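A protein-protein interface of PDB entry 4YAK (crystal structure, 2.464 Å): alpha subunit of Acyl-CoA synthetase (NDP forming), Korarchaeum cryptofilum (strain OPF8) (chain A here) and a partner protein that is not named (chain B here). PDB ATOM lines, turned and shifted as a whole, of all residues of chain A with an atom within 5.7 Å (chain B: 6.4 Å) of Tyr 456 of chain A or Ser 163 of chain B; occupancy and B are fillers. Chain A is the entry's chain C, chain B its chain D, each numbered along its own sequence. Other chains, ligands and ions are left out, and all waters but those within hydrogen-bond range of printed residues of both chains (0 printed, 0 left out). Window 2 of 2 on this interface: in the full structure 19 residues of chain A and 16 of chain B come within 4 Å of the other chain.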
ATOM      1  N   LYS A 270      -2.234  11.050  16.067  1.00  0.00           N
ATOM      2  CA  LYS A 270      -1.388  11.409  14.937  1.00  0.00           C
ATOM      3  C   LYS A 270      -0.718  10.165  14.358  1.00  0.00           C
ATOM      4  O   LYS A 270      -0.678   9.974  13.138  1.00  0.00           O
ATOM      5  CB  LYS A 270      -0.329  12.432  15.345  1.00  0.00           C
ATOM      6  CG  LYS A 270       0.451  12.985  14.162  1.00  0.00           C
ATOM      7  CD  LYS A 270       1.541  13.966  14.575  1.00  0.00           C
ATOM      8  CE  LYS A 270       0.979  15.199  15.247  1.00  0.00           C
ATOM      9  NZ  LYS A 270       2.023  16.248  15.421  1.00  0.00           N
ATOM     10  N   GLN A 271      -0.199   9.309  15.232  1.00  0.00           N
ATOM     11  CA  GLN A 271       0.465   8.087  14.776  1.00  0.00           C
ATOM     12  C   GLN A 271      -0.506   7.105  14.113  1.00  0.00           C
ATOM     13  O   GLN A 271      -0.080   6.203  13.394  1.00  0.00           O
ATOM     14  CB  GLN A 271       1.179   7.397  15.935  1.00  0.00           C
ATOM     15  CG  GLN A 271       2.233   8.251  16.602  1.00  0.00           C
ATOM     16  CD  GLN A 271       2.944   7.527  17.734  1.00  0.00           C
ATOM     17  OE1 GLN A 271       2.874   7.941  18.890  1.00  0.00           O
ATOM     18  NE2 GLN A 271       3.640   6.451  17.404  1.00  0.00           N
ATOM     19  N   GLY A 273      -3.035   8.193  12.156  1.00  0.00           N
ATOM     20  CA  GLY A 273      -3.606   8.880  11.006  1.00  0.00           C
ATOM     21  C   GLY A 273      -5.052   9.296  11.234  1.00  0.00           C
ATOM     22  O   GLY A 273      -5.844   9.412  10.293  1.00  0.00           O
ATOM     23  N   ALA A 451      -5.578  13.141   3.772  1.00  0.00           N
ATOM     24  CA  ALA A 451      -4.502  12.845   2.834  1.00  0.00           C
ATOM     25  C   ALA A 451      -3.161  12.892   3.558  1.00  0.00           C
ATOM     26  O   ALA A 451      -2.389  11.938   3.522  1.00  0.00           O
ATOM     27  CB  ALA A 451      -4.510  13.823   1.688  1.00  0.00           C
ATOM     28  N   ARG A 452      -2.907  13.999   4.239  1.00  0.00           N
ATOM     29  CA  ARG A 452      -1.651  14.181   4.956  1.00  0.00           C
ATOM     30  C   ARG A 452      -1.508  13.209   6.125  1.00  0.00           C
ATOM     31  O   ARG A 452      -0.399  12.790   6.462  1.00  0.00           O
ATOM     32  CB  ARG A 452      -1.545  15.628   5.442  1.00  0.00           C
ATOM     33  CG  ARG A 452      -1.387  16.614   4.297  1.00  0.00           C
ATOM     34  CD  ARG A 452      -1.563  18.047   4.729  1.00  0.00           C
ATOM     35  NE  ARG A 452      -1.639  18.933   3.566  1.00  0.00           N
ATOM     36  CZ  ARG A 452      -1.853  20.245   3.630  1.00  0.00           C
ATOM     37  NH1 ARG A 452      -2.015  20.847   4.804  1.00  0.00           N
ATOM     38  NH2 ARG A 452      -1.902  20.956   2.513  1.00  0.00           N
ATOM     39  N   ALA A 453      -2.634  12.821   6.717  1.00  0.00           N
ATOM     40  CA  ALA A 453      -2.629  11.849   7.809  1.00  0.00           C
ATOM     41  C   ALA A 453      -2.299  10.455   7.278  1.00  0.00           C
ATOM     42  O   ALA A 453      -1.568   9.693   7.912  1.00  0.00           O
ATOM     43  CB  ALA A 453      -3.972  11.839   8.522  1.00  0.00           C
ATOM     44  N   ARG A 454      -2.842  10.129   6.112  1.00  0.00           N
ATOM     45  CA  ARG A 454      -2.577   8.848   5.466  1.00  0.00           C
ATOM     46  C   ARG A 454      -1.102   8.758   5.098  1.00  0.00           C
ATOM     47  O   ARG A 454      -0.446   7.741   5.327  1.00  0.00           O
ATOM     48  CB  ARG A 454      -3.467   8.686   4.224  1.00  0.00           C
ATOM     49  CG  ARG A 454      -3.255   7.413   3.460  1.00  0.00           C
ATOM     50  CD  ARG A 454      -4.075   7.376   2.182  1.00  0.00           C
ATOM     51  NE  ARG A 454      -5.471   7.030   2.431  1.00  0.00           N
ATOM     52  CZ  ARG A 454      -6.389   6.883   1.478  1.00  0.00           C
ATOM     53  NH1 ARG A 454      -6.067   7.067   0.202  1.00  0.00           N
ATOM     54  NH2 ARG A 454      -7.642   6.559   1.798  1.00  0.00           N
ATOM     55  N   SER A 455      -0.587   9.840   4.531  1.00  0.00           N
ATOM     56  CA  SER A 455       0.816   9.943   4.171  1.00  0.00           C
ATOM     57  C   SER A 455       1.717   9.767   5.395  1.00  0.00           C
ATOM     58  O   SER A 455       2.814   9.223   5.301  1.00  0.00           O
ATOM     59  CB  SER A 455       1.085  11.293   3.505  1.00  0.00           C
ATOM     60  OG  SER A 455       2.464  11.479   3.259  1.00  0.00           O
ATOM     61  N   TYR A 456       1.259  10.247   6.545  1.00  0.00           N
ATOM     62  CA  TYR A 456       2.057  10.131   7.761  1.00  0.00           C
ATOM     63  C   TYR A 456       2.226   8.666   8.112  1.00  0.00           C
ATOM     64  O   TYR A 456       3.320   8.205   8.425  1.00  0.00           O
ATOM     65  CB  TYR A 456       1.407  10.886   8.928  1.00  0.00           C
ATOM     66  CG  TYR A 456       2.210  10.829  10.211  1.00  0.00           C
ATOM     67  CD1 TYR A 456       2.220   9.685  10.997  1.00  0.00           C
ATOM     68  CD2 TYR A 456       2.952  11.918  10.635  1.00  0.00           C
ATOM     69  CE1 TYR A 456       2.956   9.621  12.168  1.00  0.00           C
ATOM     70  CE2 TYR A 456       3.687  11.872  11.802  1.00  0.00           C
ATOM     71  CZ  TYR A 456       3.689  10.719  12.567  1.00  0.00           C
ATOM     72  OH  TYR A 456       4.424  10.668  13.736  1.00  0.00           O
ATOM     73  N   VAL A 457       1.130   7.931   8.040  1.00  0.00           N
ATOM     74  CA  VAL A 457       1.156   6.531   8.393  1.00  0.00           C
ATOM     75  C   VAL A 457       1.965   5.730   7.383  1.00  0.00           C
ATOM     76  O   VAL A 457       2.732   4.851   7.770  1.00  0.00           O
ATOM     77  CB  VAL A 457      -0.261   5.970   8.487  1.00  0.00           C
ATOM     78  CG1 VAL A 457      -0.228   4.471   8.711  1.00  0.00           C
ATOM     79  CG2 VAL A 457      -1.023   6.674   9.593  1.00  0.00           C
ATOM     80  N   MET A 458       1.804   6.037   6.098  1.00  0.00           N
ATOM     81  CA  MET A 458       2.576   5.379   5.052  1.00  0.00           C
ATOM     82  C   MET A 458       4.071   5.516   5.300  1.00  0.00           C
ATOM     83  O   MET A 458       4.810   4.539   5.200  1.00  0.00           O
ATOM     84  CB  MET A 458       2.213   5.946   3.679  1.00  0.00           C
ATOM     85  CG  MET A 458       0.974   5.303   3.053  1.00  0.00           C
ATOM     86  SD  MET A 458      -0.004   6.413   1.998  1.00  0.00           S
ATOM     87  CE  MET A 458       1.277   7.244   1.057  1.00  0.00           C
ATOM     88  N   LYS A 459       4.523   6.719   5.626  1.00  0.00           N
ATOM     89  CA  LYS A 459       5.941   6.930   5.892  1.00  0.00           C
ATOM     90  C   LYS A 459       6.350   6.209   7.177  1.00  0.00           C
ATOM     91  O   LYS A 459       7.475   5.724   7.304  1.00  0.00           O
ATOM     92  CB  LYS A 459       6.266   8.419   6.007  1.00  0.00           C
ATOM     93  CG  LYS A 459       6.081   9.218   4.722  1.00  0.00           C
ATOM     94  CD  LYS A 459       6.733  10.592   4.858  1.00  0.00           C
ATOM     95  CE  LYS A 459       6.282  11.553   3.786  1.00  0.00           C
ATOM     96  NZ  LYS A 459       5.001  12.205   4.171  1.00  0.00           N
ATOM     97  N   SER A 460       5.412   6.109   8.112  1.00  0.00           N
ATOM     98  CA  SER A 460       5.678   5.492   9.394  1.00  0.00           C
ATOM     99  C   SER A 460       5.841   3.978   9.266  1.00  0.00           C
ATOM    100  O   SER A 460       6.553   3.360  10.062  1.00  0.00           O
ATOM    101  CB  SER A 460       4.552   5.824  10.367  1.00  0.00           C
ATOM    102  OG  SER A 460       4.911   5.452  11.678  1.00  0.00           O
ATOM    103  N   LEU A 461       5.176   3.390   8.274  1.00  0.00           N
ATOM    104  CA  LEU A 461       5.292   1.961   7.972  1.00  0.00           C
ATOM    105  C   LEU A 461       6.335   1.629   6.907  1.00  0.00           C
ATOM    106  O   LEU A 461       6.524   0.455   6.580  1.00  0.00           O
ATOM    107  CB  LEU A 461       3.943   1.382   7.538  1.00  0.00           C
ATOM    108  CG  LEU A 461       2.886   1.091   8.604  1.00  0.00           C
ATOM    109  CD1 LEU A 461       3.142   1.817   9.901  1.00  0.00           C
ATOM    110  CD2 LEU A 461       1.490   1.381   8.061  1.00  0.00           C
ATOM    111  N   SER B 150       7.265  17.035  23.345  1.00  0.00           N
ATOM    112  CA  SER B 150       6.465  16.237  22.427  1.00  0.00           C
ATOM    113  C   SER B 150       6.519  14.765  22.839  1.00  0.00           C
ATOM    114  O   SER B 150       7.462  14.335  23.498  1.00  0.00           O
ATOM    115  CB  SER B 150       6.965  16.418  21.001  1.00  0.00           C
ATOM    116  OG  SER B 150       8.327  16.061  20.932  1.00  0.00           O
ATOM    117  N   ARG B 152       5.727  10.542  21.578  1.00  0.00           N
ATOM    118  CA  ARG B 152       5.423   9.513  20.591  1.00  0.00           C
ATOM    119  C   ARG B 152       5.410   8.158  21.280  1.00  0.00           C
ATOM    120  O   ARG B 152       6.253   7.886  22.133  1.00  0.00           O
ATOM    121  CB  ARG B 152       6.442   9.524  19.451  1.00  0.00           C
ATOM    122  CG  ARG B 152       6.319  10.697  18.500  1.00  0.00           C
ATOM    123  CD  ARG B 152       4.967  10.705  17.783  1.00  0.00           C
ATOM    124  NE  ARG B 152       4.950  11.667  16.687  1.00  0.00           N
ATOM    125  CZ  ARG B 152       4.828  12.981  16.843  1.00  0.00           C
ATOM    126  NH1 ARG B 152       4.710  13.499  18.053  1.00  0.00           N
ATOM    127  NH2 ARG B 152       4.829  13.782  15.786  1.00  0.00           N
ATOM    128  N   SER B 157       9.082   4.944  14.518  1.00  0.00           N
ATOM    129  CA  SER B 157       9.584   4.944  13.157  1.00  0.00           C
ATOM    130  C   SER B 157      10.445   6.183  12.963  1.00  0.00           C
ATOM    131  O   SER B 157      10.405   7.098  13.780  1.00  0.00           O
ATOM    132  CB  SER B 157       8.436   4.944  12.154  1.00  0.00           C
ATOM    133  OG  SER B 157       7.712   6.162  12.220  1.00  0.00           O
ATOM    134  N   GLU B 158      11.200   6.227  11.870  1.00  0.00           N
ATOM    135  CA  GLU B 158      12.005   7.404  11.553  1.00  0.00           C
ATOM    136  C   GLU B 158      11.096   8.624  11.355  1.00  0.00           C
ATOM    137  O   GLU B 158      11.460   9.747  11.698  1.00  0.00           O
ATOM    138  CB  GLU B 158      12.855   7.147  10.305  1.00  0.00           C
ATOM    139  CG  GLU B 158      13.694   8.337   9.860  1.00  0.00           C
ATOM    140  CD  GLU B 158      14.604   8.015   8.679  1.00  0.00           C
ATOM    141  OE1 GLU B 158      14.582   6.861   8.191  1.00  0.00           O
ATOM    142  OE2 GLU B 158      15.347   8.922   8.243  1.00  0.00           O
ATOM    143  N   GLN B 159       9.901   8.383  10.827  1.00  0.00           N
ATOM    144  CA  GLN B 159       8.912   9.441  10.616  1.00  0.00           C
ATOM    145  C   GLN B 159       8.452  10.029  11.944  1.00  0.00           C
ATOM    146  O   GLN B 159       8.342  11.247  12.090  1.00  0.00           O
ATOM    147  CB  GLN B 159       7.712   8.892   9.833  1.00  0.00           C
ATOM    148  CG  GLN B 159       6.516   9.831   9.749  1.00  0.00           C
ATOM    149  CD  GLN B 159       6.820  11.104   8.997  1.00  0.00           C
ATOM    150  OE1 GLN B 159       7.788  11.181   8.241  1.00  0.00           O
ATOM    151  NE2 GLN B 159       5.998  12.116   9.210  1.00  0.00           N
ATOM    152  N   ASP B 160       8.183   9.157  12.911  1.00  0.00           N
ATOM    153  CA  ASP B 160       7.780   9.588  14.243  1.00  0.00           C
ATOM    154  C   ASP B 160       8.869  10.457  14.864  1.00  0.00           C
ATOM    155  O   ASP B 160       8.596  11.532  15.394  1.00  0.00           O
ATOM    156  CB  ASP B 160       7.503   8.382  15.152  1.00  0.00           C
ATOM    157  CG  ASP B 160       6.260   7.613  14.753  1.00  0.00           C
ATOM    158  OD1 ASP B 160       5.288   8.250  14.299  1.00  0.00           O
ATOM    159  OD2 ASP B 160       6.249   6.371  14.909  1.00  0.00           O
ATOM    160  N   ALA B 161      10.106   9.978  14.801  1.00  0.00           N
ATOM    161  CA  ALA B 161      11.231  10.703  15.376  1.00  0.00           C
ATOM    162  C   ALA B 161      11.362  12.088  14.747  1.00  0.00           C
ATOM    163  O   ALA B 161      11.394  13.096  15.445  1.00  0.00           O
ATOM    164  CB  ALA B 161      12.524   9.903  15.199  1.00  0.00           C
ATOM    165  N   GLU B 162      11.379  12.138  13.419  1.00  0.00           N
ATOM    166  CA  GLU B 162      11.579  13.401  12.722  1.00  0.00           C
ATOM    167  C   GLU B 162      10.509  14.412  13.073  1.00  0.00           C
ATOM    168  O   GLU B 162      10.818  15.574  13.321  1.00  0.00           O
ATOM    169  CB  GLU B 162      11.589  13.193  11.214  1.00  0.00           C
ATOM    170  CG  GLU B 162      11.807  14.485  10.441  1.00  0.00           C
ATOM    171  CD  GLU B 162      12.128  14.258   8.981  1.00  0.00           C
ATOM    172  OE1 GLU B 162      12.832  13.272   8.661  1.00  0.00           O
ATOM    173  OE2 GLU B 162      11.671  15.075   8.151  1.00  0.00           O
ATOM    174  N   SER B 163       9.254  13.972  13.099  1.00  0.00           N
ATOM    175  CA  SER B 163       8.137  14.892  13.296  1.00  0.00           C
ATOM    176  C   SER B 163       8.005  15.383  14.748  1.00  0.00           C
ATOM    177  O   SER B 163       7.648  16.543  14.987  1.00  0.00           O
ATOM    178  CB  SER B 163       6.829  14.234  12.823  1.00  0.00           C
ATOM    179  OG  SER B 163       6.418  13.162  13.649  1.00  0.00           O
ATOM    180  N   MET B 164       8.318  14.532  15.718  1.00  0.00           N
ATOM    181  CA  MET B 164       8.191  14.941  17.117  1.00  0.00           C
ATOM    182  C   MET B 164       9.268  15.968  17.459  1.00  0.00           C
ATOM    183  O   MET B 164       9.096  16.790  18.360  1.00  0.00           O
ATOM    184  CB  MET B 164       8.266  13.729  18.051  1.00  0.00           C
ATOM    185  CG  MET B 164       9.667  13.305  18.447  1.00  0.00           C
ATOM    186  SD  MET B 164       9.669  11.775  19.413  1.00  0.00           S
ATOM    187  CE  MET B 164       8.963  12.346  20.959  1.00  0.00           C
ATOM    188  N   ILE B 165      10.362  15.950  16.708  1.00  0.00           N
ATOM    189  CA  ILE B 165      11.401  16.947  16.884  1.00  0.00           C
ATOM    190  C   ILE B 165      10.916  18.303  16.393  1.00  0.00           C
ATOM    191  O   ILE B 165      11.142  19.317  17.047  1.00  0.00           O
ATOM    192  CB  ILE B 165      12.687  16.562  16.139  1.00  0.00           C
ATOM    193  CG1 ILE B 165      13.328  15.348  16.809  1.00  0.00           C
ATOM    194  CG2 ILE B 165      13.680  17.729  16.124  1.00  0.00           C
ATOM    195  CD1 ILE B 165      14.493  14.762  16.029  1.00  0.00           C
ATOM    196  N   LYS B 166      10.237  18.318  15.250  1.00  0.00           N
ATOM    197  CA  LYS B 166       9.749  19.564  14.665  1.00  0.00           C
ATOM    198  C   LYS B 166       8.492  20.083  15.358  1.00  0.00           C
ATOM    199  O   LYS B 166       8.150  21.259  15.235  1.00  0.00           O
ATOM    200  CB  LYS B 166       9.492  19.370  13.173  1.00  0.00           C
ATOM    201  CG  LYS B 166      10.754  19.031  12.406  1.00  0.00           C
ATOM    202  CD  LYS B 166      10.484  18.759  10.948  1.00  0.00           C
ATOM    203  CE  LYS B 166      11.793  18.612  10.193  1.00  0.00           C
ATOM    204  NZ  LYS B 166      11.605  18.028   8.840  1.00  0.00           N
ATOM    205  N   GLU B 167       7.814  19.207  16.093  1.00  0.00           N
ATOM    206  CA  GLU B 167       6.629  19.586  16.860  1.00  0.00           C
ATOM    207  C   GLU B 167       6.911  20.695  17.880  1.00  0.00           C
ATOM    208  O   GLU B 167       6.153  21.655  17.972  1.00  0.00           O
ATOM    209  CB  GLU B 167       6.068  18.371  17.612  1.00  0.00           C
ATOM    210  CG  GLU B 167       4.867  17.698  16.977  1.00  0.00           C
ATOM    211  CD  GLU B 167       4.062  16.863  17.977  1.00  0.00           C
ATOM    212  OE1 GLU B 167       2.987  16.338  17.605  1.00  0.00           O
ATOM    213  OE2 GLU B 167       4.501  16.731  19.142  1.00  0.00           O
ATOM    214  N   VAL B 168       7.992  20.558  18.651  1.00  0.00           N
ATOM    215  CA  VAL B 168       8.254  21.484  19.757  1.00  0.00           C
ATOM    216  C   VAL B 168       8.461  22.901  19.260  1.00  0.00           C
ATOM    217  O   VAL B 168       9.020  23.117  18.187  1.00  0.00           O
ATOM    218  CB  VAL B 168       9.493  21.071  20.596  1.00  0.00           C
ATOM    219  CG1 VAL B 168       9.262  19.723  21.260  1.00  0.00           C
ATOM    220  CG2 VAL B 168      10.747  21.034  19.740  1.00  0.00           C
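Tyr 456 of chain A touches just these residues of chain B: Arg 152 (3.2 Å), Gln 159 (3.4 Å), Asp 160 (2.6 Å) and Ser 163 (3.2 Å).
Printed residues of chain B within 4 Å of Ser 460 of chain A: Ser 157 (2.9 Å), Gln 159 (3.99 Å) and Asp 160 (3.6 Å).
Printed residues of chain A within 4 Å of Glu 167 of chain B: Lys 270.
Ala 453 of chain A touches none of the printed residues of chain B.
The nearest residue of chain A that does not touch Ser 163 of chain B is Lys 270 of chain A (5.0 Å).
NZ of Lys 459 of chain A lies within hydrogen-bond range of OG of Ser 455 of chain A (2.8 Å).
NH2 of Arg 152 of chain B lies within hydrogen-bond range of OG of Ser 163 of chain B (2.7 Å).
NH1 of Arg 152 of chain B lies within salt-bridge range of OE1 of Glu 167 of chain B.
OG of Ser 157 of chain B sits at hydrogen-bond distance from OD2 of Asp 160 of chain B, 3.1 Å away.
OG of Ser 163 of chain B lies within hydrogen-bond range of O of Gln 159 of chain B (3.1 Å).
The side-chain hydroxyl of Ser 163 of chain B sits at hydrogen-bond distance from the backbone carbonyl oxygen of Asp 160 of chain B (3.2 Å).
Lys 270 of chain A touches Arg 152 of chain B.
Arg 152 of chain B touches Gln 271 of chain A.
Gln 271 of chain A touches Asp 160 of chain B.
NE2 of Gln 159 of chain B touches CD2 of Tyr 456 of chain A, at 3.4 Å.
Lys 459 of chain A touches Gln 159 of chain B (CD to OE1, 3.6 Å).
Ser 460 of chain A touches Gln 159 of chain B (CA to CB, 3.99 Å).
Ser 460 of chain A touches Asp 160 of chain B.
The guanidinium group of Arg 152 of chain B is in hydrogen-bond range of the side-chain hydroxyl of Tyr 456 of chain A.
OD1 of Asp 160 of chain B is in hydrogen-bond range of OH of Tyr 456 of chain A.
The side-chain hydroxyl of Ser 163 of chain B lies within hydrogen-bond range of the side-chain hydroxyl of Tyr 456 of chain A, at 3.2 Å.
OG of Ser 460 of chain A sits at hydrogen-bond distance from OG of Ser 157 of chain B.
NZ of Lys 270 of chain A lies close to OE1 of Glu 167 of chain B (2.4 Å).
Hydrophobic or aromatic side chains of chain A that line the printed part of chain B: Tyr 456.
Among the printed residues, 12 pairs touch across the chains.
Among the printed residues, Asp or Glu carboxylates within 4 Å of a Lys or Arg side-chain nitrogen of the other chain: Lys 270 of chain A with Glu 167 of chain B.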
